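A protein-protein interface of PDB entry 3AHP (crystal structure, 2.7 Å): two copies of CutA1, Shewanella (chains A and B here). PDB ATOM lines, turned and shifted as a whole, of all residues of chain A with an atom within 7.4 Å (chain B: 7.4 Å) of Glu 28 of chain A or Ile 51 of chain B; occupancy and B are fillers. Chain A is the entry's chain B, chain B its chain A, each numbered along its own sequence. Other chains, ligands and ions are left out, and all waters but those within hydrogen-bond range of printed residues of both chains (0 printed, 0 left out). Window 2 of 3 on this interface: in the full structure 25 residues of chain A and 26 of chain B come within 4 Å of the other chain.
Hydrophobic or aromatic side chains of chain A within 4 Å of the printed part of chain B: Ala 23 and Val 27. Among the printed residues, 7 pairs touch across the chains.
No position is printed for both chains. Of the 7 pairs that touch across the chains among the printed residues, none has its exchanged pair printed and touching as well.
CB of Ala 23 of chain A touches CD1 of Ile 44 of chain B (3.9 Å). Ile 44 of chain B touches Val 27 of chain A (O to CG2, 3.5 Å). Val 27 of chain A touches Tyr 45 of chain B (CG1 to C, 3.8 Å). Val 27 of chain A touches Gln 46 of chain B. CD1 of Ile 51 of chain B touches OE1 of Glu 28 of chain A (3.6 Å).
The backbone carbonyl oxygen (O) of Tyr 45 of chain B is in hydrogen-bond range of the backbone NH (N) of Cys 52 of chain B.
The side-chain amide oxygen (OD1) of Asn 49 of chain B lies within hydrogen-bond range of the side-chain amino group (NZ) of Lys 30 of chain A, at 3.1 Å. The side-chain amino group (NZ) of Lys 30 of chain A sits close to the side-chain amide nitrogen (NE2) of Gln 46 of chain B, 3.1 Å away.
Glu 28 of chain A touches one residue of chain B. Of the printed residues of chain A, Ile 51 of chain B touches Glu 28 (3.6 Å). Printed residues of chain A within 4 Å of Ile 44 of chain B: Ala 23 (3.9 Å) and Val 27 (3.5 Å). Printed residues of chain A within 4 Å of Asn 49 of chain B: Lys 30 (3.1 Å). Of the printed residues of chain B, Ala 23 of chain A touches Ile 44 (3.9 Å). Of the printed residues of chain A, Tyr 45 of chain B touches Val 27. Asn 50 of chain B touches none of the printed residues of chain A. Leu 31 of chain A touches none of the printed residues of chain B. The nearest residue of chain A that does not touch Ile 51 of chain B is Thr 24 of chain A (4.6 Å).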
ATOM      1  N   ARG A  21       0.108   7.674 -20.646  1.00  0.00           N
ATOM      2  CA  ARG A  21       0.350   8.315 -19.378  1.00  0.00           C
ATOM      3  C   ARG A  21      -0.977   8.637 -18.665  1.00  0.00           C
ATOM      4  O   ARG A  21      -1.148   8.319 -17.493  1.00  0.00           O
ATOM      5  CB  ARG A  21       1.199   9.566 -19.611  1.00  0.00           C
ATOM      6  CG  ARG A  21       1.940  10.097 -18.386  1.00  0.00           C
ATOM      7  CD  ARG A  21       3.185  10.928 -18.780  1.00  0.00           C
ATOM      8  NE  ARG A  21       2.858  12.302 -19.189  1.00  0.00           N
ATOM      9  CZ  ARG A  21       3.206  12.847 -20.357  1.00  0.00           C
ATOM     10  NH1 ARG A  21       3.901  12.138 -21.254  1.00  0.00           N
ATOM     11  NH2 ARG A  21       2.846  14.097 -20.635  1.00  0.00           N
ATOM     12  N   ILE A  22      -1.909   9.262 -19.376  1.00  0.00           N
ATOM     13  CA  ILE A  22      -3.222   9.556 -18.837  1.00  0.00           C
ATOM     14  C   ILE A  22      -4.021   8.288 -18.548  1.00  0.00           C
ATOM     15  O   ILE A  22      -4.571   8.148 -17.460  1.00  0.00           O
ATOM     16  CB  ILE A  22      -4.017  10.531 -19.749  1.00  0.00           C
ATOM     17  CG1 ILE A  22      -3.241  11.848 -19.913  1.00  0.00           C
ATOM     18  CG2 ILE A  22      -5.416  10.800 -19.179  1.00  0.00           C
ATOM     19  CD1 ILE A  22      -3.706  12.747 -21.053  1.00  0.00           C
ATOM     20  N   ALA A  23      -4.083   7.357 -19.499  1.00  0.00           N
ATOM     21  CA  ALA A  23      -4.671   6.030 -19.212  1.00  0.00           C
ATOM     22  C   ALA A  23      -4.176   5.400 -17.894  1.00  0.00           C
ATOM     23  O   ALA A  23      -4.982   5.016 -17.040  1.00  0.00           O
ATOM     24  CB  ALA A  23      -4.425   5.061 -20.372  1.00  0.00           C
ATOM     25  N   THR A  24      -2.856   5.267 -17.764  1.00  0.00           N
ATOM     26  CA  THR A  24      -2.229   4.705 -16.573  1.00  0.00           C
ATOM     27  C   THR A  24      -2.676   5.429 -15.289  1.00  0.00           C
ATOM     28  O   THR A  24      -3.113   4.804 -14.324  1.00  0.00           O
ATOM     29  CB  THR A  24      -0.672   4.675 -16.709  1.00  0.00           C
ATOM     30  OG1 THR A  24      -0.305   3.881 -17.836  1.00  0.00           O
ATOM     31  CG2 THR A  24      -0.018   4.086 -15.492  1.00  0.00           C
ATOM     32  N   ALA A  25      -2.624   6.750 -15.300  1.00  0.00           N
ATOM     33  CA  ALA A  25      -3.062   7.508 -14.152  1.00  0.00           C
ATOM     34  C   ALA A  25      -4.507   7.139 -13.811  1.00  0.00           C
ATOM     35  O   ALA A  25      -4.831   6.739 -12.690  1.00  0.00           O
ATOM     36  CB  ALA A  25      -2.911   9.016 -14.419  1.00  0.00           C
ATOM     37  N   LEU A  26      -5.371   7.270 -14.805  1.00  0.00           N
ATOM     38  CA  LEU A  26      -6.778   6.959 -14.660  1.00  0.00           C
ATOM     39  C   LEU A  26      -6.964   5.585 -14.039  1.00  0.00           C
ATOM     40  O   LEU A  26      -7.745   5.418 -13.107  1.00  0.00           O
ATOM     41  CB  LEU A  26      -7.440   6.999 -16.035  1.00  0.00           C
ATOM     42  CG  LEU A  26      -8.445   8.117 -16.277  1.00  0.00           C
ATOM     43  CD1 LEU A  26      -8.349   9.215 -15.233  1.00  0.00           C
ATOM     44  CD2 LEU A  26      -8.283   8.645 -17.669  1.00  0.00           C
ATOM     45  N   VAL A  27      -6.241   4.601 -14.557  1.00  0.00           N
ATOM     46  CA  VAL A  27      -6.407   3.250 -14.062  1.00  0.00           C
ATOM     47  C   VAL A  27      -5.784   3.020 -12.693  1.00  0.00           C
ATOM     48  O   VAL A  27      -6.460   2.548 -11.792  1.00  0.00           O
ATOM     49  CB  VAL A  27      -6.086   2.157 -15.123  1.00  0.00           C
ATOM     50  CG1 VAL A  27      -5.761   0.823 -14.477  1.00  0.00           C
ATOM     51  CG2 VAL A  27      -7.276   1.982 -16.041  1.00  0.00           C
ATOM     52  N   GLU A  28      -4.572   3.510 -12.467  1.00  0.00           N
ATOM     53  CA  GLU A  28      -4.041   3.435 -11.111  1.00  0.00           C
ATOM     54  C   GLU A  28      -4.671   4.263  -9.999  1.00  0.00           C
ATOM     55  O   GLU A  28      -4.640   3.861  -8.850  1.00  0.00           O
ATOM     56  CB  GLU A  28      -2.528   3.175 -10.992  1.00  0.00           C
ATOM     57  CG  GLU A  28      -1.573   4.207 -11.525  1.00  0.00           C
ATOM     58  CD  GLU A  28      -0.125   3.931 -11.070  1.00  0.00           C
ATOM     59  OE1 GLU A  28       0.076   3.036 -10.216  1.00  0.00           O
ATOM     60  OE2 GLU A  28       0.814   4.602 -11.556  1.00  0.00           O
ATOM     61  N   ALA A  29      -5.427   5.287 -10.364  1.00  0.00           N
ATOM     62  CA  ALA A  29      -6.232   6.028  -9.389  1.00  0.00           C
ATOM     63  C   ALA A  29      -7.544   5.318  -9.150  1.00  0.00           C
ATOM     64  O   ALA A  29      -8.365   5.763  -8.350  1.00  0.00           O
ATOM     65  CB  ALA A  29      -6.483   7.464  -9.867  1.00  0.00           C
ATOM     66  N   LYS A  30      -7.763   4.250  -9.913  1.00  0.00           N
ATOM     67  CA  LYS A  30      -9.035   3.533  -9.920  1.00  0.00           C
ATOM     68  C   LYS A  30     -10.221   4.469 -10.186  1.00  0.00           C
ATOM     69  O   LYS A  30     -11.290   4.320  -9.587  1.00  0.00           O
ATOM     70  CB  LYS A  30      -9.242   2.794  -8.597  1.00  0.00           C
ATOM     71  CG  LYS A  30      -8.196   1.715  -8.279  1.00  0.00           C
ATOM     72  CD  LYS A  30      -8.484   1.099  -6.897  1.00  0.00           C
ATOM     73  CE  LYS A  30      -7.229   0.540  -6.237  1.00  0.00           C
ATOM     74  NZ  LYS A  30      -7.021  -0.905  -6.536  1.00  0.00           N
ATOM     75  N   LEU A  31     -10.046   5.418 -11.104  1.00  0.00           N
ATOM     76  CA  LEU A  31     -11.156   6.253 -11.527  1.00  0.00           C
ATOM     77  C   LEU A  31     -11.901   5.650 -12.716  1.00  0.00           C
ATOM     78  O   LEU A  31     -13.120   5.744 -12.830  1.00  0.00           O
ATOM     79  CB  LEU A  31     -10.668   7.664 -11.808  1.00  0.00           C
ATOM     80  CG  LEU A  31     -10.316   8.347 -10.485  1.00  0.00           C
ATOM     81  CD1 LEU A  31      -9.432   9.567 -10.667  1.00  0.00           C
ATOM     82  CD2 LEU A  31     -11.583   8.690  -9.683  1.00  0.00           C
ATOM     83  N   ALA A  32     -11.165   4.931 -13.540  1.00  0.00           N
ATOM     84  CA  ALA A  32     -11.744   4.233 -14.651  1.00  0.00           C
ATOM     85  C   ALA A  32     -11.319   2.791 -14.499  1.00  0.00           C
ATOM     86  O   ALA A  32     -10.140   2.516 -14.261  1.00  0.00           O
ATOM     87  CB  ALA A  32     -11.218   4.805 -15.969  1.00  0.00           C
ATOM     88  N   ILE B  44      -6.392  -0.810 -21.274  1.00  0.00           N
ATOM     89  CA  ILE B  44      -5.635  -0.694 -20.034  1.00  0.00           C
ATOM     90  C   ILE B  44      -6.595  -0.782 -18.862  1.00  0.00           C
ATOM     91  O   ILE B  44      -7.595  -0.072 -18.819  1.00  0.00           O
ATOM     92  CB  ILE B  44      -4.857   0.638 -19.989  1.00  0.00           C
ATOM     93  CG1 ILE B  44      -4.044   0.817 -21.270  1.00  0.00           C
ATOM     94  CG2 ILE B  44      -3.986   0.735 -18.758  1.00  0.00           C
ATOM     95  CD1 ILE B  44      -2.805   1.617 -21.095  1.00  0.00           C
ATOM     96  N   TYR B  45      -6.302  -1.695 -17.939  1.00  0.00           N
ATOM     97  CA  TYR B  45      -7.238  -2.094 -16.881  1.00  0.00           C
ATOM     98  C   TYR B  45      -6.487  -2.730 -15.697  1.00  0.00           C
ATOM     99  O   TYR B  45      -5.316  -3.100 -15.825  1.00  0.00           O
ATOM    100  CB  TYR B  45      -8.289  -3.069 -17.440  1.00  0.00           C
ATOM    101  CG  TYR B  45      -7.705  -4.379 -17.938  1.00  0.00           C
ATOM    102  CD1 TYR B  45      -7.627  -5.487 -17.102  1.00  0.00           C
ATOM    103  CD2 TYR B  45      -7.189  -4.494 -19.229  1.00  0.00           C
ATOM    104  CE1 TYR B  45      -7.062  -6.672 -17.531  1.00  0.00           C
ATOM    105  CE2 TYR B  45      -6.621  -5.681 -19.670  1.00  0.00           C
ATOM    106  CZ  TYR B  45      -6.556  -6.766 -18.809  1.00  0.00           C
ATOM    107  OH  TYR B  45      -5.998  -7.953 -19.219  1.00  0.00           O
ATOM    108  N   GLN B  46      -7.169  -2.860 -14.556  1.00  0.00           N
ATOM    109  CA  GLN B  46      -6.574  -3.418 -13.342  1.00  0.00           C
ATOM    110  C   GLN B  46      -7.162  -4.806 -13.056  1.00  0.00           C
ATOM    111  O   GLN B  46      -8.386  -4.965 -13.061  1.00  0.00           O
ATOM    112  CB  GLN B  46      -6.824  -2.468 -12.156  1.00  0.00           C
ATOM    113  CG  GLN B  46      -5.869  -2.637 -10.958  1.00  0.00           C
ATOM    114  CD  GLN B  46      -5.548  -1.325 -10.220  1.00  0.00           C
ATOM    115  OE1 GLN B  46      -4.398  -0.885 -10.179  1.00  0.00           O
ATOM    116  NE2 GLN B  46      -6.558  -0.732  -9.599  1.00  0.00           N
ATOM    117  N   TRP B  47      -6.299  -5.808 -12.849  1.00  0.00           N
ATOM    118  CA  TRP B  47      -6.751  -7.201 -12.646  1.00  0.00           C
ATOM    119  C   TRP B  47      -6.345  -7.842 -11.320  1.00  0.00           C
ATOM    120  O   TRP B  47      -7.156  -8.523 -10.685  1.00  0.00           O
ATOM    121  CB  TRP B  47      -6.338  -8.127 -13.803  1.00  0.00           C
ATOM    122  CG  TRP B  47      -6.901  -9.547 -13.672  1.00  0.00           C
ATOM    123  CD1 TRP B  47      -8.180  -9.892 -13.309  1.00  0.00           C
ATOM    124  CD2 TRP B  47      -6.205 -10.793 -13.912  1.00  0.00           C
ATOM    125  NE1 TRP B  47      -8.319 -11.264 -13.305  1.00  0.00           N
ATOM    126  CE2 TRP B  47      -7.126 -11.840 -13.666  1.00  0.00           C
ATOM    127  CE3 TRP B  47      -4.898 -11.122 -14.315  1.00  0.00           C
ATOM    128  CZ2 TRP B  47      -6.778 -13.194 -13.795  1.00  0.00           C
ATOM    129  CZ3 TRP B  47      -4.554 -12.467 -14.448  1.00  0.00           C
ATOM    130  CH2 TRP B  47      -5.492 -13.485 -14.186  1.00  0.00           C
ATOM    131  N   ASP B  48      -5.068  -7.728 -10.963  1.00  0.00           N
ATOM    132  CA  ASP B  48      -4.578  -8.279  -9.696  1.00  0.00           C
ATOM    133  C   ASP B  48      -4.319  -7.162  -8.684  1.00  0.00           C
ATOM    134  O   ASP B  48      -3.455  -7.288  -7.817  1.00  0.00           O
ATOM    135  CB  ASP B  48      -3.295  -9.107  -9.913  1.00  0.00           C
ATOM    136  CG  ASP B  48      -3.272 -10.396  -9.080  1.00  0.00           C
ATOM    137  OD1 ASP B  48      -4.127 -11.276  -9.322  1.00  0.00           O
ATOM    138  OD2 ASP B  48      -2.393 -10.540  -8.198  1.00  0.00           O
ATOM    139  N   ASN B  49      -5.037  -6.052  -8.823  1.00  0.00           N
ATOM    140  CA  ASN B  49      -4.552  -4.796  -8.277  1.00  0.00           C
ATOM    141  C   ASN B  49      -3.253  -4.391  -8.998  1.00  0.00           C
ATOM    142  O   ASN B  49      -2.451  -3.595  -8.476  1.00  0.00           O
ATOM    143  CB  ASN B  49      -4.313  -4.941  -6.766  1.00  0.00           C
ATOM    144  CG  ASN B  49      -4.926  -3.809  -5.967  1.00  0.00           C
ATOM    145  OD1 ASN B  49      -4.522  -2.652  -6.099  1.00  0.00           O
ATOM    146  ND2 ASN B  49      -5.911  -4.135  -5.140  1.00  0.00           N
ATOM    147  N   ASN B  50      -3.049  -4.975 -10.186  1.00  0.00           N
ATOM    148  CA  ASN B  50      -1.934  -4.635 -11.083  1.00  0.00           C
ATOM    149  C   ASN B  50      -2.414  -4.089 -12.441  1.00  0.00           C
ATOM    150  O   ASN B  50      -3.507  -4.414 -12.904  1.00  0.00           O
ATOM    151  CB  ASN B  50      -1.035  -5.856 -11.314  1.00  0.00           C
ATOM    152  CG  ASN B  50      -0.077  -6.108 -10.167  1.00  0.00           C
ATOM    153  OD1 ASN B  50      -0.209  -7.091  -9.441  1.00  0.00           O
ATOM    154  ND2 ASN B  50       0.910  -5.234 -10.016  1.00  0.00           N
ATOM    155  N   ILE B  51      -1.551  -3.315 -13.097  1.00  0.00           N
ATOM    156  CA  ILE B  51      -1.893  -2.603 -14.325  1.00  0.00           C
ATOM    157  C   ILE B  51      -1.619  -3.481 -15.548  1.00  0.00           C
ATOM    158  O   ILE B  51      -0.477  -3.831 -15.811  1.00  0.00           O
ATOM    159  CB  ILE B  51      -1.051  -1.298 -14.451  1.00  0.00           C
ATOM    160  CG1 ILE B  51      -1.365  -0.331 -13.297  1.00  0.00           C
ATOM    161  CG2 ILE B  51      -1.250  -0.640 -15.824  1.00  0.00           C
ATOM    162  CD1 ILE B  51      -0.127   0.389 -12.710  1.00  0.00           C
ATOM    163  N   CYS B  52      -2.657  -3.790 -16.321  1.00  0.00           N
ATOM    164  CA  CYS B  52      -2.510  -4.696 -17.462  1.00  0.00           C
ATOM    165  C   CYS B  52      -2.717  -4.025 -18.805  1.00  0.00           C
ATOM    166  O   CYS B  52      -3.418  -3.023 -18.912  1.00  0.00           O
ATOM    167  CB  CYS B  52      -3.449  -5.891 -17.340  1.00  0.00           C
ATOM    168  SG  CYS B  52      -3.162  -6.878 -15.866  1.00  0.00           S
ATOM    169  N   GLN B  53      -2.179  -4.656 -19.837  1.00  0.00           N
ATOM    170  CA  GLN B  53      -2.177  -4.109 -21.178  1.00  0.00           C
ATOM    171  C   GLN B  53      -2.425  -5.247 -22.171  1.00  0.00           C
ATOM    172  O   GLN B  53      -1.506  -5.996 -22.514  1.00  0.00           O
ATOM    173  CB  GLN B  53      -0.819  -3.463 -21.449  1.00  0.00           C
ATOM    174  CG  GLN B  53      -0.827  -2.279 -22.403  1.00  0.00           C
ATOM    175  CD  GLN B  53       0.428  -1.404 -22.266  1.00  0.00           C
ATOM    176  OE1 GLN B  53       1.437  -1.826 -21.699  1.00  0.00           O
ATOM    177  NE2 GLN B  53       0.355  -0.175 -22.771  1.00  0.00           N
